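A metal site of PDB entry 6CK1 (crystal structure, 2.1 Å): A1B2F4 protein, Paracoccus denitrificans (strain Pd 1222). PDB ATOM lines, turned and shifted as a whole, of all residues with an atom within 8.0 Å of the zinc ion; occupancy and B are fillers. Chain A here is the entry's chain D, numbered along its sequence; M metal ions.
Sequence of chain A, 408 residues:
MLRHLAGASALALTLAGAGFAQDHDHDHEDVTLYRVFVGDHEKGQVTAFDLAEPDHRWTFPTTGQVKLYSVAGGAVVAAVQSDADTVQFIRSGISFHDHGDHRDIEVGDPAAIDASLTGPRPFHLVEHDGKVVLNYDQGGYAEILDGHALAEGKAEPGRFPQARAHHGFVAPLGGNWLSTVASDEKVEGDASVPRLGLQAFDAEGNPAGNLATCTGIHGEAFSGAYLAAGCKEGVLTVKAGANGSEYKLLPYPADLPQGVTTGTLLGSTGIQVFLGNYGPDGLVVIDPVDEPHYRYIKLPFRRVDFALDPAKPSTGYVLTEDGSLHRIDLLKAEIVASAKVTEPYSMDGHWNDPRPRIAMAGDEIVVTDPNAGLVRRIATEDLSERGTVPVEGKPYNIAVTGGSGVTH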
ATOM      1  N   HIS A  28      23.292 -34.312  28.974  1.00  0.00           N
ATOM      2  CA  HIS A  28      24.268 -34.125  27.898  1.00  0.00           C
ATOM      3  C   HIS A  28      24.144 -35.270  26.896  1.00  0.00           C
ATOM      4  O   HIS A  28      24.421 -36.422  27.231  1.00  0.00           O
ATOM      5  CB  HIS A  28      25.683 -34.049  28.461  1.00  0.00           C
ATOM      6  CG  HIS A  28      26.761 -34.038  27.420  1.00  0.00           C
ATOM      7  ND1 HIS A  28      27.220 -35.192  26.819  1.00  0.00           N
ATOM      8  CD2 HIS A  28      27.448 -33.024  26.856  1.00  0.00           C
ATOM      9  CE1 HIS A  28      28.160 -34.884  25.938  1.00  0.00           C
ATOM     10  NE2 HIS A  28      28.313 -33.576  25.941  1.00  0.00           N
ATOM     11  N   GLU A  29      23.743 -34.952  25.664  1.00  0.00           N
ATOM     12  CA  GLU A  29      23.470 -35.969  24.656  1.00  0.00           C
ATOM     13  C   GLU A  29      24.036 -35.525  23.312  1.00  0.00           C
ATOM     14  O   GLU A  29      23.752 -34.419  22.859  1.00  0.00           O
ATOM     15  CB  GLU A  29      21.956 -36.218  24.526  1.00  0.00           C
ATOM     16  CG  GLU A  29      21.585 -37.626  24.094  1.00  0.00           C
ATOM     17  CD  GLU A  29      21.645 -38.621  25.250  1.00  0.00           C
ATOM     18  OE1 GLU A  29      21.021 -38.349  26.302  1.00  0.00           O
ATOM     19  OE2 GLU A  29      22.330 -39.659  25.102  1.00  0.00           O
ATOM     20  N   HIS A  97      24.518 -23.669  17.904  1.00  0.00           N
ATOM     21  CA  HIS A  97      24.851 -22.512  18.734  1.00  0.00           C
ATOM     22  C   HIS A  97      26.126 -22.844  19.511  1.00  0.00           C
ATOM     23  O   HIS A  97      26.158 -23.829  20.261  1.00  0.00           O
ATOM     24  CB  HIS A  97      23.687 -22.160  19.684  1.00  0.00           C
ATOM     25  CG  HIS A  97      22.379 -21.981  18.995  1.00  0.00           C
ATOM     26  ND1 HIS A  97      21.967 -20.776  18.462  1.00  0.00           N
ATOM     27  CD2 HIS A  97      21.378 -22.865  18.736  1.00  0.00           C
ATOM     28  CE1 HIS A  97      20.779 -20.913  17.902  1.00  0.00           C
ATOM     29  NE2 HIS A  97      20.392 -22.176  18.056  1.00  0.00           N
ATOM     30  N   ASP A  98      27.160 -22.028  19.328  1.00  0.00           N
ATOM     31  CA  ASP A  98      28.400 -22.248  20.077  1.00  0.00           C
ATOM     32  C   ASP A  98      28.093 -22.360  21.563  1.00  0.00           C
ATOM     33  O   ASP A  98      27.214 -21.680  22.089  1.00  0.00           O
ATOM     34  CB  ASP A  98      29.390 -21.104  19.833  1.00  0.00           C
ATOM     35  CG  ASP A  98      29.983 -21.128  18.437  1.00  0.00           C
ATOM     36  OD1 ASP A  98      29.452 -21.846  17.567  1.00  0.00           O
ATOM     37  OD2 ASP A  98      30.998 -20.434  18.215  1.00  0.00           O
ATOM     38  N   HIS A  99      28.852 -23.220  22.248  1.00  0.00           N
ATOM     39  CA  HIS A  99      28.632 -23.401  23.662  1.00  0.00           C
ATOM     40  C   HIS A  99      29.956 -23.728  24.353  1.00  0.00           C
ATOM     41  O   HIS A  99      30.105 -24.748  25.008  1.00  0.00           O
ATOM     42  CB  HIS A  99      27.562 -24.465  23.899  1.00  0.00           C
ATOM     43  CG  HIS A  99      26.909 -24.358  25.250  1.00  0.00           C
ATOM     44  ND1 HIS A  99      26.127 -25.352  25.788  1.00  0.00           N
ATOM     45  CD2 HIS A  99      26.945 -23.367  26.171  1.00  0.00           C
ATOM     46  CE1 HIS A  99      25.705 -24.985  26.984  1.00  0.00           C
ATOM     47  NE2 HIS A  99      26.175 -23.777  27.236  1.00  0.00           N
ATOM     48  N   GLY A 100      30.936 -22.834  24.236  1.00  0.00           N
ATOM     49  CA  GLY A 100      32.249 -23.075  24.807  1.00  0.00           C
ATOM     50  C   GLY A 100      32.998 -24.257  24.199  1.00  0.00           C
ATOM     51  O   GLY A 100      33.666 -24.118  23.167  1.00  0.00           O
ATOM     52  N   ASP A 101      32.891 -25.419  24.840  1.00  0.00           N
ATOM     53  CA  ASP A 101      33.557 -26.646  24.380  1.00  0.00           C
ATOM     54  C   ASP A 101      33.035 -27.141  23.045  1.00  0.00           C
ATOM     55  O   ASP A 101      33.749 -27.849  22.326  1.00  0.00           O
ATOM     56  CB  ASP A 101      33.330 -27.759  25.401  1.00  0.00           C
ATOM     57  CG  ASP A 101      34.509 -27.982  26.286  1.00  0.00           C
ATOM     58  OD1 ASP A 101      35.629 -27.817  25.757  1.00  0.00           O
ATOM     59  OD2 ASP A 101      34.315 -28.300  27.480  1.00  0.00           O
ATOM     60  N   HIS A 102      31.777 -26.854  22.729  1.00  0.00           N
ATOM     61  CA  HIS A 102      31.001 -27.615  21.758  1.00  0.00           C
ATOM     62  C   HIS A 102      29.925 -26.704  21.192  1.00  0.00           C
ATOM     63  O   HIS A 102      29.843 -25.524  21.539  1.00  0.00           O
ATOM     64  CB  HIS A 102      30.367 -28.855  22.409  1.00  0.00           C
ATOM     65  CG  HIS A 102      29.452 -28.526  23.552  1.00  0.00           C
ATOM     66  ND1 HIS A 102      29.891 -28.416  24.847  1.00  0.00           N
ATOM     67  CD2 HIS A 102      28.125 -28.250  23.574  1.00  0.00           C
ATOM     68  CE1 HIS A 102      28.873 -28.086  25.626  1.00  0.00           C
ATOM     69  NE2 HIS A 102      27.791 -27.988  24.885  1.00  0.00           N
ATOM     70  N   ARG A 103      29.107 -27.268  20.305  1.00  0.00           N
ATOM     71  CA  ARG A 103      27.923 -26.630  19.751  1.00  0.00           C
ATOM     72  C   ARG A 103      26.682 -27.345  20.263  1.00  0.00           C
ATOM     73  O   ARG A 103      26.659 -28.580  20.344  1.00  0.00           O
ATOM     74  CB  ARG A 103      27.932 -26.665  18.226  1.00  0.00           C
ATOM     75  CG  ARG A 103      28.453 -28.011  17.665  1.00  0.00           C
ATOM     76  CD  ARG A 103      27.769 -28.486  16.337  1.00  0.00           C
ATOM     77  NE  ARG A 103      28.173 -27.716  15.174  1.00  0.00           N
ATOM     78  CZ  ARG A 103      28.251 -28.174  13.922  1.00  0.00           C
ATOM     79  NH1 ARG A 103      27.976 -29.438  13.620  1.00  0.00           N
ATOM     80  NH2 ARG A 103      28.650 -27.359  12.947  1.00  0.00           N
ATOM     81  N   ASP A 104      25.651 -26.587  20.593  1.00  0.00           N
ATOM     82  CA  ASP A 104      24.328 -27.155  20.812  1.00  0.00           C
ATOM     83  C   ASP A 104      23.565 -27.148  19.502  1.00  0.00           C
ATOM     84  O   ASP A 104      23.690 -26.231  18.688  1.00  0.00           O
ATOM     85  CB  ASP A 104      23.544 -26.385  21.867  1.00  0.00           C
ATOM     86  CG  ASP A 104      24.076 -26.623  23.285  1.00  0.00           C
ATOM     87  OD1 ASP A 104      24.958 -27.473  23.486  1.00  0.00           O
ATOM     88  OD2 ASP A 104      23.530 -25.981  24.203  1.00  0.00           O
ATOM     89  N   ILE A 105      22.716 -28.163  19.311  1.00  0.00           N
ATOM     90  CA  ILE A 105      21.881 -28.301  18.126  1.00  0.00           C
ATOM     91  C   ILE A 105      20.446 -27.966  18.500  1.00  0.00           C
ATOM     92  O   ILE A 105      19.952 -28.411  19.537  1.00  0.00           O
ATOM     93  CB  ILE A 105      21.986 -29.703  17.507  1.00  0.00           C
ATOM     94  CG1 ILE A 105      21.144 -29.766  16.221  1.00  0.00           C
ATOM     95  CG2 ILE A 105      21.519 -30.773  18.471  1.00  0.00           C
ATOM     96  CD1 ILE A 105      21.253 -31.087  15.532  1.00  0.00           C
ATOM     97  N   GLY A 405      25.815 -32.245  17.101  1.00  0.00           N
ATOM     98  CA  GLY A 405      25.808 -31.245  18.151  1.00  0.00           C
ATOM     99  C   GLY A 405      25.346 -31.893  19.436  1.00  0.00           C
ATOM    100  O   GLY A 405      25.203 -33.114  19.508  1.00  0.00           O
ATOM    101  N   VAL A 406      25.152 -31.059  20.455  1.00  0.00           N
ATOM    102  CA  VAL A 406      24.732 -31.497  21.784  1.00  0.00           C
ATOM    103  C   VAL A 406      23.343 -30.993  22.135  1.00  0.00           C
ATOM    104  O   VAL A 406      22.931 -29.907  21.718  1.00  0.00           O
ATOM    105  CB  VAL A 406      25.741 -31.007  22.842  1.00  0.00           C
ATOM    106  CG1 VAL A 406      25.323 -31.458  24.209  1.00  0.00           C
ATOM    107  CG2 VAL A 406      27.123 -31.567  22.533  1.00  0.00           C
ATOM    108  N   THR A 407      22.614 -31.805  22.896  1.00  0.00           N
ATOM    109  CA  THR A 407      21.380 -31.398  23.563  1.00  0.00           C
ATOM    110  C   THR A 407      21.582 -31.642  25.060  1.00  0.00           C
ATOM    111  O   THR A 407      22.285 -32.570  25.446  1.00  0.00           O
ATOM    112  CB  THR A 407      20.158 -32.163  23.066  1.00  0.00           C
ATOM    113  OG1 THR A 407      20.299 -33.546  23.406  1.00  0.00           O
ATOM    114  CG2 THR A 407      19.989 -32.030  21.547  1.00  0.00           C
ATOM    115  N   HIS A 408      20.982 -30.812  25.897  1.00  0.00           N
ATOM    116  CA  HIS A 408      21.193 -30.947  27.339  1.00  0.00           C
ATOM    117  C   HIS A 408      19.949 -31.435  28.074  1.00  0.00           C
ATOM    118  O   HIS A 408      19.868 -32.607  28.422  1.00  0.00           O
ATOM    119  CB  HIS A 408      21.667 -29.625  27.932  1.00  0.00           C
ATOM    120  CG  HIS A 408      23.026 -29.198  27.453  1.00  0.00           C
ATOM    121  ND1 HIS A 408      24.195 -29.744  27.947  1.00  0.00           N
ATOM    122  CD2 HIS A 408      23.393 -28.309  26.505  1.00  0.00           C
ATOM    123  CE1 HIS A 408      25.219 -29.188  27.342  1.00  0.00           C
ATOM    124  NE2 HIS A 408      24.764 -28.319  26.454  1.00  0.00           N
ATOM    125  OXT HIS A 408      18.999 -30.689  28.349  1.00  0.00           O
HETATM  126 ZN    ZN M   1      25.809 -27.228  25.225  1.00  0.00          ZN
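Along chain A the residues within 4 Å of the zinc ion span positions 99 to 408. The nearest printed residue that does not touch the zinc ion is Val 406 (4.4 Å).
NE2 of His 408 is bound to the zinc ion, 1.9 Å away. The side-chain carboxylate (OD1) of Asp 104 is bound to the zinc ion, at 2.0 Å. ND1 of His 99 binds the zinc ion (2.0 Å). The zinc ion is bound by a ring nitrogen (NE2) of His 102. The zinc ion has four donor atoms within binding distance. Slightly farther from the zinc ion lies OD2 of Asp 104 (2.8 Å).
N of His 97 lies within hydrogen-bond range of O of Asp 104 (2.8 Å).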
